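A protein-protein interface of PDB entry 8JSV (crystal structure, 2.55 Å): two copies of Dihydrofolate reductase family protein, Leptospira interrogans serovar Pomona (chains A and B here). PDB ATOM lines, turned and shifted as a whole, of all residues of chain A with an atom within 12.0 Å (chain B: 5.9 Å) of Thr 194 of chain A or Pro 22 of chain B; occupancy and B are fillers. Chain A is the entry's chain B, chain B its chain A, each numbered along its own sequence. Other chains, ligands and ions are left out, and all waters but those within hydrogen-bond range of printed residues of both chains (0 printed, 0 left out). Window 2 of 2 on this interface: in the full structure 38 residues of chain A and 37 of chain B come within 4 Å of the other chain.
The backbone carbonyl oxygen (O) of Gly 34 of chain B lies within hydrogen-bond range of the backbone NH (N) of Gly 193 of chain A.
The backbone NH (N) of Val 195 of chain A sits at hydrogen-bond distance from the backbone carbonyl oxygen (O) of Gly 20 of chain B (3.0 Å).
The side-chain carboxylate (OE1) of Glu 24 of chain B is in hydrogen-bond range of the backbone NH (N) of Gly 20 of chain B (2.8 Å).
The backbone carbonyl oxygen of Ala 18 of chain B sits at hydrogen-bond distance from the backbone NH of Gly 34 of chain B, at 3.0 Å.
The backbone carbonyl oxygen of Gly 21 of chain B sits close to the backbone NH of Gly 34 of chain B (3.5 Å).
Among the printed residues, merely in contact across the chains: Gly 193 of chain A with Ala 37 of chain B (3.3 Å), Thr 192 of chain A with Gly 33 of chain B (3.3 Å), Thr 192 of chain A with Tyr 32 of chain B (3.4 Å), Thr 192 of chain A with Gly 34 of chain B (3.4 Å), Thr 194 of chain A with Pro 22 of chain B (3.4 Å), Gly 193 of chain A with Pro 22 of chain B (3.5 Å), Thr 194 of chain A with Gly 20 of chain B (3.7 Å), Thr 194 of chain A with Ala 37 of chain B (3.9 Å) and Gly 193 of chain A with Gly 21 of chain B (3.96 Å).
Printed residues of chain B within 4 Å of Thr 194 of chain A: Gly 20, Pro 22 and Ala 37.
Pro 22 of chain B touches just these residues of chain A: Gly 193 (3.5 Å) and Thr 194 (3.4 Å).
Gly 20 of chain B touches just these residues of chain A: Thr 194 and Val 195.
No residue of chain A comes within 4 Å of Glu 23 of chain B.
No residue of chain A comes within 4 Å of Thr 26 of chain B.
Printed residues of chain A within 4 Å of Gly 33 of chain B: Thr 192.
Gly 34 of chain B touches just these residues of chain A: Thr 192 and Gly 193.
Of chain A, only Gly 193 and Thr 194 come within 4 Å of Ala 37 of chain B.
Of the printed residues of chain B, Val 195 of chain A touches Gly 20 (3.0 Å).
Of the printed residues of chain B, Thr 192 of chain A touches Tyr 32, Gly 33 and Gly 34.
Lys 191 of chain A touches none of the printed residues of chain B.
The nearest printed residue of chain A that does not touch Tyr 32 of chain B is Val 190 of chain A (4.3 Å).
Printed residues of chain A that touch a printed residue of chain B: Thr 192, Gly 193, Thr 194 and Val 195.
Hydrophobic or aromatic side chains of chain A within 4 Å of the printed part of chain B: Val 195.
Printed residues of chain B that touch a printed residue of chain A: Gly 20, Gly 21, Pro 22, Tyr 32, Gly 33, Gly 34 and Ala 37.
Among the printed residues, no Asp or Glu carboxylate lies within 4 Å of a Lys or Arg side-chain nitrogen of the other chain.
No position is printed for both chains.
Of the 11 pairs that touch across the chains among the printed residues, none has its exchanged pair printed and touching as well.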
ATOM      1  N   VAL A 190      -2.061  -3.948  30.153  1.00  0.00           N
ATOM      2  CA  VAL A 190      -1.290  -4.793  29.239  1.00  0.00           C
ATOM      3  C   VAL A 190      -2.103  -5.069  27.986  1.00  0.00           C
ATOM      4  O   VAL A 190      -3.231  -5.587  28.049  1.00  0.00           O
ATOM      5  CB  VAL A 190      -0.881  -6.120  29.898  1.00  0.00           C
ATOM      6  CG1 VAL A 190       0.290  -6.733  29.122  1.00  0.00           C
ATOM      7  CG2 VAL A 190      -0.551  -5.930  31.381  1.00  0.00           C
ATOM      8  N   LYS A 191      -1.517  -4.749  26.843  1.00  0.00           N
ATOM      9  CA  LYS A 191      -2.124  -5.018  25.555  1.00  0.00           C
ATOM     10  C   LYS A 191      -1.406  -6.195  24.912  1.00  0.00           C
ATOM     11  O   LYS A 191      -0.176  -6.314  25.003  1.00  0.00           O
ATOM     12  CB  LYS A 191      -2.072  -3.779  24.648  1.00  0.00           C
ATOM     13  CG  LYS A 191      -3.243  -2.799  24.861  1.00  0.00           C
ATOM     14  CD  LYS A 191      -4.522  -3.516  25.362  1.00  0.00           C
ATOM     15  CE  LYS A 191      -5.597  -2.531  25.873  1.00  0.00           C
ATOM     16  NZ  LYS A 191      -6.131  -1.636  24.794  1.00  0.00           N
ATOM     17  N   THR A 192      -2.192  -7.087  24.306  1.00  0.00           N
ATOM     18  CA  THR A 192      -1.693  -8.196  23.507  1.00  0.00           C
ATOM     19  C   THR A 192      -2.254  -8.081  22.101  1.00  0.00           C
ATOM     20  O   THR A 192      -3.359  -7.568  21.900  1.00  0.00           O
ATOM     21  CB  THR A 192      -2.098  -9.559  24.087  1.00  0.00           C
ATOM     22  OG1 THR A 192      -3.528  -9.651  24.118  1.00  0.00           O
ATOM     23  CG2 THR A 192      -1.534  -9.749  25.501  1.00  0.00           C
ATOM     24  N   GLY A 193      -1.483  -8.567  21.134  1.00  0.00           N
ATOM     25  CA  GLY A 193      -1.964  -8.731  19.776  1.00  0.00           C
ATOM     26  C   GLY A 193      -1.428 -10.021  19.200  1.00  0.00           C
ATOM     27  O   GLY A 193      -1.209 -10.975  19.955  1.00  0.00           O
ATOM     28  N   THR A 194      -1.209 -10.069  17.882  1.00  0.00           N
ATOM     29  CA  THR A 194      -0.519 -11.180  17.234  1.00  0.00           C
ATOM     30  C   THR A 194       0.588 -10.620  16.353  1.00  0.00           C
ATOM     31  O   THR A 194       0.324  -9.780  15.490  1.00  0.00           O
ATOM     32  CB  THR A 194      -1.479 -12.018  16.388  1.00  0.00           C
ATOM     33  OG1 THR A 194      -2.316 -12.836  17.231  1.00  0.00           O
ATOM     34  CG2 THR A 194      -0.693 -12.895  15.417  1.00  0.00           C
ATOM     35  N   VAL A 195       1.811 -11.082  16.554  1.00  0.00           N
ATOM     36  CA  VAL A 195       2.926 -10.625  15.724  1.00  0.00           C
ATOM     37  C   VAL A 195       2.791 -11.057  14.270  1.00  0.00           C
ATOM     38  O   VAL A 195       2.593 -12.232  13.985  1.00  0.00           O
ATOM     39  CB  VAL A 195       4.250 -11.112  16.289  1.00  0.00           C
ATOM     40  CG1 VAL A 195       5.385 -10.257  15.773  1.00  0.00           C
ATOM     41  CG2 VAL A 195       4.201 -11.046  17.792  1.00  0.00           C
ATOM     42  N   ALA B  18       5.200 -17.107  25.759  1.00  0.00           N
ATOM     43  CA  ALA B  18       4.238 -16.700  24.744  1.00  0.00           C
ATOM     44  C   ALA B  18       4.358 -15.231  24.301  1.00  0.00           C
ATOM     45  O   ALA B  18       3.392 -14.483  24.343  1.00  0.00           O
ATOM     46  CB  ALA B  18       2.828 -16.977  25.250  1.00  0.00           C
ATOM     47  N   GLY B  20       4.582 -14.050  21.262  1.00  0.00           N
ATOM     48  CA  GLY B  20       4.129 -13.726  19.923  1.00  0.00           C
ATOM     49  C   GLY B  20       2.645 -13.812  19.630  1.00  0.00           C
ATOM     50  O   GLY B  20       2.190 -13.262  18.622  1.00  0.00           O
ATOM     51  N   GLY B  21       1.874 -14.480  20.481  1.00  0.00           N
ATOM     52  CA  GLY B  21       0.455 -14.561  20.248  1.00  0.00           C
ATOM     53  C   GLY B  21      -0.318 -15.219  21.370  1.00  0.00           C
ATOM     54  O   GLY B  21       0.215 -15.959  22.204  1.00  0.00           O
ATOM     55  N   PRO B  22      -1.625 -14.961  21.385  1.00  0.00           N
ATOM     56  CA  PRO B  22      -2.452 -15.381  22.527  1.00  0.00           C
ATOM     57  C   PRO B  22      -2.407 -16.860  22.801  1.00  0.00           C
ATOM     58  O   PRO B  22      -2.610 -17.275  23.949  1.00  0.00           O
ATOM     59  CB  PRO B  22      -3.866 -14.950  22.121  1.00  0.00           C
ATOM     60  CG  PRO B  22      -3.679 -13.945  21.051  1.00  0.00           C
ATOM     61  CD  PRO B  22      -2.393 -14.245  20.358  1.00  0.00           C
ATOM     62  N   GLU B  23      -2.196 -17.679  21.779  1.00  0.00           N
ATOM     63  CA  GLU B  23      -2.246 -19.120  21.968  1.00  0.00           C
ATOM     64  C   GLU B  23      -0.864 -19.754  21.860  1.00  0.00           C
ATOM     65  O   GLU B  23      -0.741 -20.977  21.943  1.00  0.00           O
ATOM     66  CB  GLU B  23      -3.206 -19.750  20.961  1.00  0.00           C
ATOM     67  CG  GLU B  23      -4.681 -19.606  21.277  1.00  0.00           C
ATOM     68  CD  GLU B  23      -5.560 -20.173  20.154  1.00  0.00           C
ATOM     69  OE1 GLU B  23      -5.145 -20.096  18.951  1.00  0.00           O
ATOM     70  OE2 GLU B  23      -6.649 -20.725  20.486  1.00  0.00           O
ATOM     71  N   GLU B  24       0.181 -18.944  21.712  1.00  0.00           N
ATOM     72  CA  GLU B  24       1.508 -19.502  21.545  1.00  0.00           C
ATOM     73  C   GLU B  24       1.862 -20.486  22.653  1.00  0.00           C
ATOM     74  O   GLU B  24       2.567 -21.472  22.397  1.00  0.00           O
ATOM     75  CB  GLU B  24       2.544 -18.385  21.478  1.00  0.00           C
ATOM     76  CG  GLU B  24       3.954 -18.908  21.294  1.00  0.00           C
ATOM     77  CD  GLU B  24       4.963 -17.799  21.152  1.00  0.00           C
ATOM     78  OE1 GLU B  24       4.604 -16.759  20.555  1.00  0.00           O
ATOM     79  OE2 GLU B  24       6.112 -17.969  21.633  1.00  0.00           O
ATOM     80  N   ASP B  25       1.389 -20.247  23.880  1.00  0.00           N
ATOM     81  CA  ASP B  25       1.624 -21.186  24.981  1.00  0.00           C
ATOM     82  C   ASP B  25       0.608 -20.914  26.078  1.00  0.00           C
ATOM     83  O   ASP B  25       0.742 -19.931  26.809  1.00  0.00           O
ATOM     84  CB  ASP B  25       3.046 -21.042  25.517  1.00  0.00           C
ATOM     85  CG  ASP B  25       3.339 -21.975  26.691  1.00  0.00           C
ATOM     86  OD1 ASP B  25       2.419 -22.727  27.120  1.00  0.00           O
ATOM     87  OD2 ASP B  25       4.499 -21.957  27.182  1.00  0.00           O
ATOM     88  N   THR B  26      -0.344 -21.815  26.253  1.00  0.00           N
ATOM     89  CA  THR B  26      -1.405 -21.595  27.217  1.00  0.00           C
ATOM     90  C   THR B  26      -1.158 -22.274  28.566  1.00  0.00           C
ATOM     91  O   THR B  26      -2.120 -22.462  29.321  1.00  0.00           O
ATOM     92  CB  THR B  26      -2.745 -22.080  26.645  1.00  0.00           C
ATOM     93  OG1 THR B  26      -2.619 -23.447  26.236  1.00  0.00           O
ATOM     94  CG2 THR B  26      -3.183 -21.226  25.473  1.00  0.00           C
ATOM     95  N   PHE B  30      -2.355 -19.120  30.995  1.00  0.00           N
ATOM     96  CA  PHE B  30      -1.671 -17.870  30.715  1.00  0.00           C
ATOM     97  C   PHE B  30      -2.504 -16.959  29.829  1.00  0.00           C
ATOM     98  O   PHE B  30      -2.881 -17.328  28.711  1.00  0.00           O
ATOM     99  CB  PHE B  30      -0.341 -18.188  30.056  1.00  0.00           C
ATOM    100  CG  PHE B  30       0.510 -16.996  29.823  1.00  0.00           C
ATOM    101  CD1 PHE B  30       1.007 -16.265  30.891  1.00  0.00           C
ATOM    102  CD2 PHE B  30       0.831 -16.602  28.531  1.00  0.00           C
ATOM    103  CE1 PHE B  30       1.816 -15.157  30.675  1.00  0.00           C
ATOM    104  CE2 PHE B  30       1.655 -15.494  28.312  1.00  0.00           C
ATOM    105  CZ  PHE B  30       2.133 -14.769  29.388  1.00  0.00           C
ATOM    106  N   TYR B  32      -1.849 -13.692  28.765  1.00  0.00           N
ATOM    107  CA  TYR B  32      -1.275 -12.523  28.098  1.00  0.00           C
ATOM    108  C   TYR B  32      -0.382 -12.897  26.917  1.00  0.00           C
ATOM    109  O   TYR B  32       0.560 -12.170  26.588  1.00  0.00           O
ATOM    110  CB  TYR B  32      -0.522 -11.649  29.109  1.00  0.00           C
ATOM    111  CG  TYR B  32      -1.368 -11.309  30.333  1.00  0.00           C
ATOM    112  CD1 TYR B  32      -1.387 -12.145  31.442  1.00  0.00           C
ATOM    113  CD2 TYR B  32      -2.166 -10.172  30.362  1.00  0.00           C
ATOM    114  CE1 TYR B  32      -2.165 -11.852  32.547  1.00  0.00           C
ATOM    115  CE2 TYR B  32      -2.956  -9.877  31.466  1.00  0.00           C
ATOM    116  CZ  TYR B  32      -2.941 -10.719  32.551  1.00  0.00           C
ATOM    117  OH  TYR B  32      -3.715 -10.443  33.647  1.00  0.00           O
ATOM    118  N   GLY B  33      -0.682 -14.017  26.243  1.00  0.00           N
ATOM    119  CA  GLY B  33       0.044 -14.352  25.034  1.00  0.00           C
ATOM    120  C   GLY B  33      -0.061 -13.206  24.042  1.00  0.00           C
ATOM    121  O   GLY B  33      -1.151 -12.666  23.834  1.00  0.00           O
ATOM    122  N   GLY B  34       1.059 -12.807  23.446  1.00  0.00           N
ATOM    123  CA  GLY B  34       1.098 -11.664  22.561  1.00  0.00           C
ATOM    124  C   GLY B  34       1.533 -10.360  23.205  1.00  0.00           C
ATOM    125  O   GLY B  34       1.403  -9.308  22.573  1.00  0.00           O
ATOM    126  N   ALA B  37       3.447  -7.873  21.325  1.00  0.00           N
ATOM    127  CA  ALA B  37       2.818  -7.427  20.087  1.00  0.00           C
ATOM    128  C   ALA B  37       2.608  -5.925  19.952  1.00  0.00           C
ATOM    129  O   ALA B  37       2.485  -5.467  18.821  1.00  0.00           O
ATOM    130  CB  ALA B  37       1.485  -8.137  19.863  1.00  0.00           C
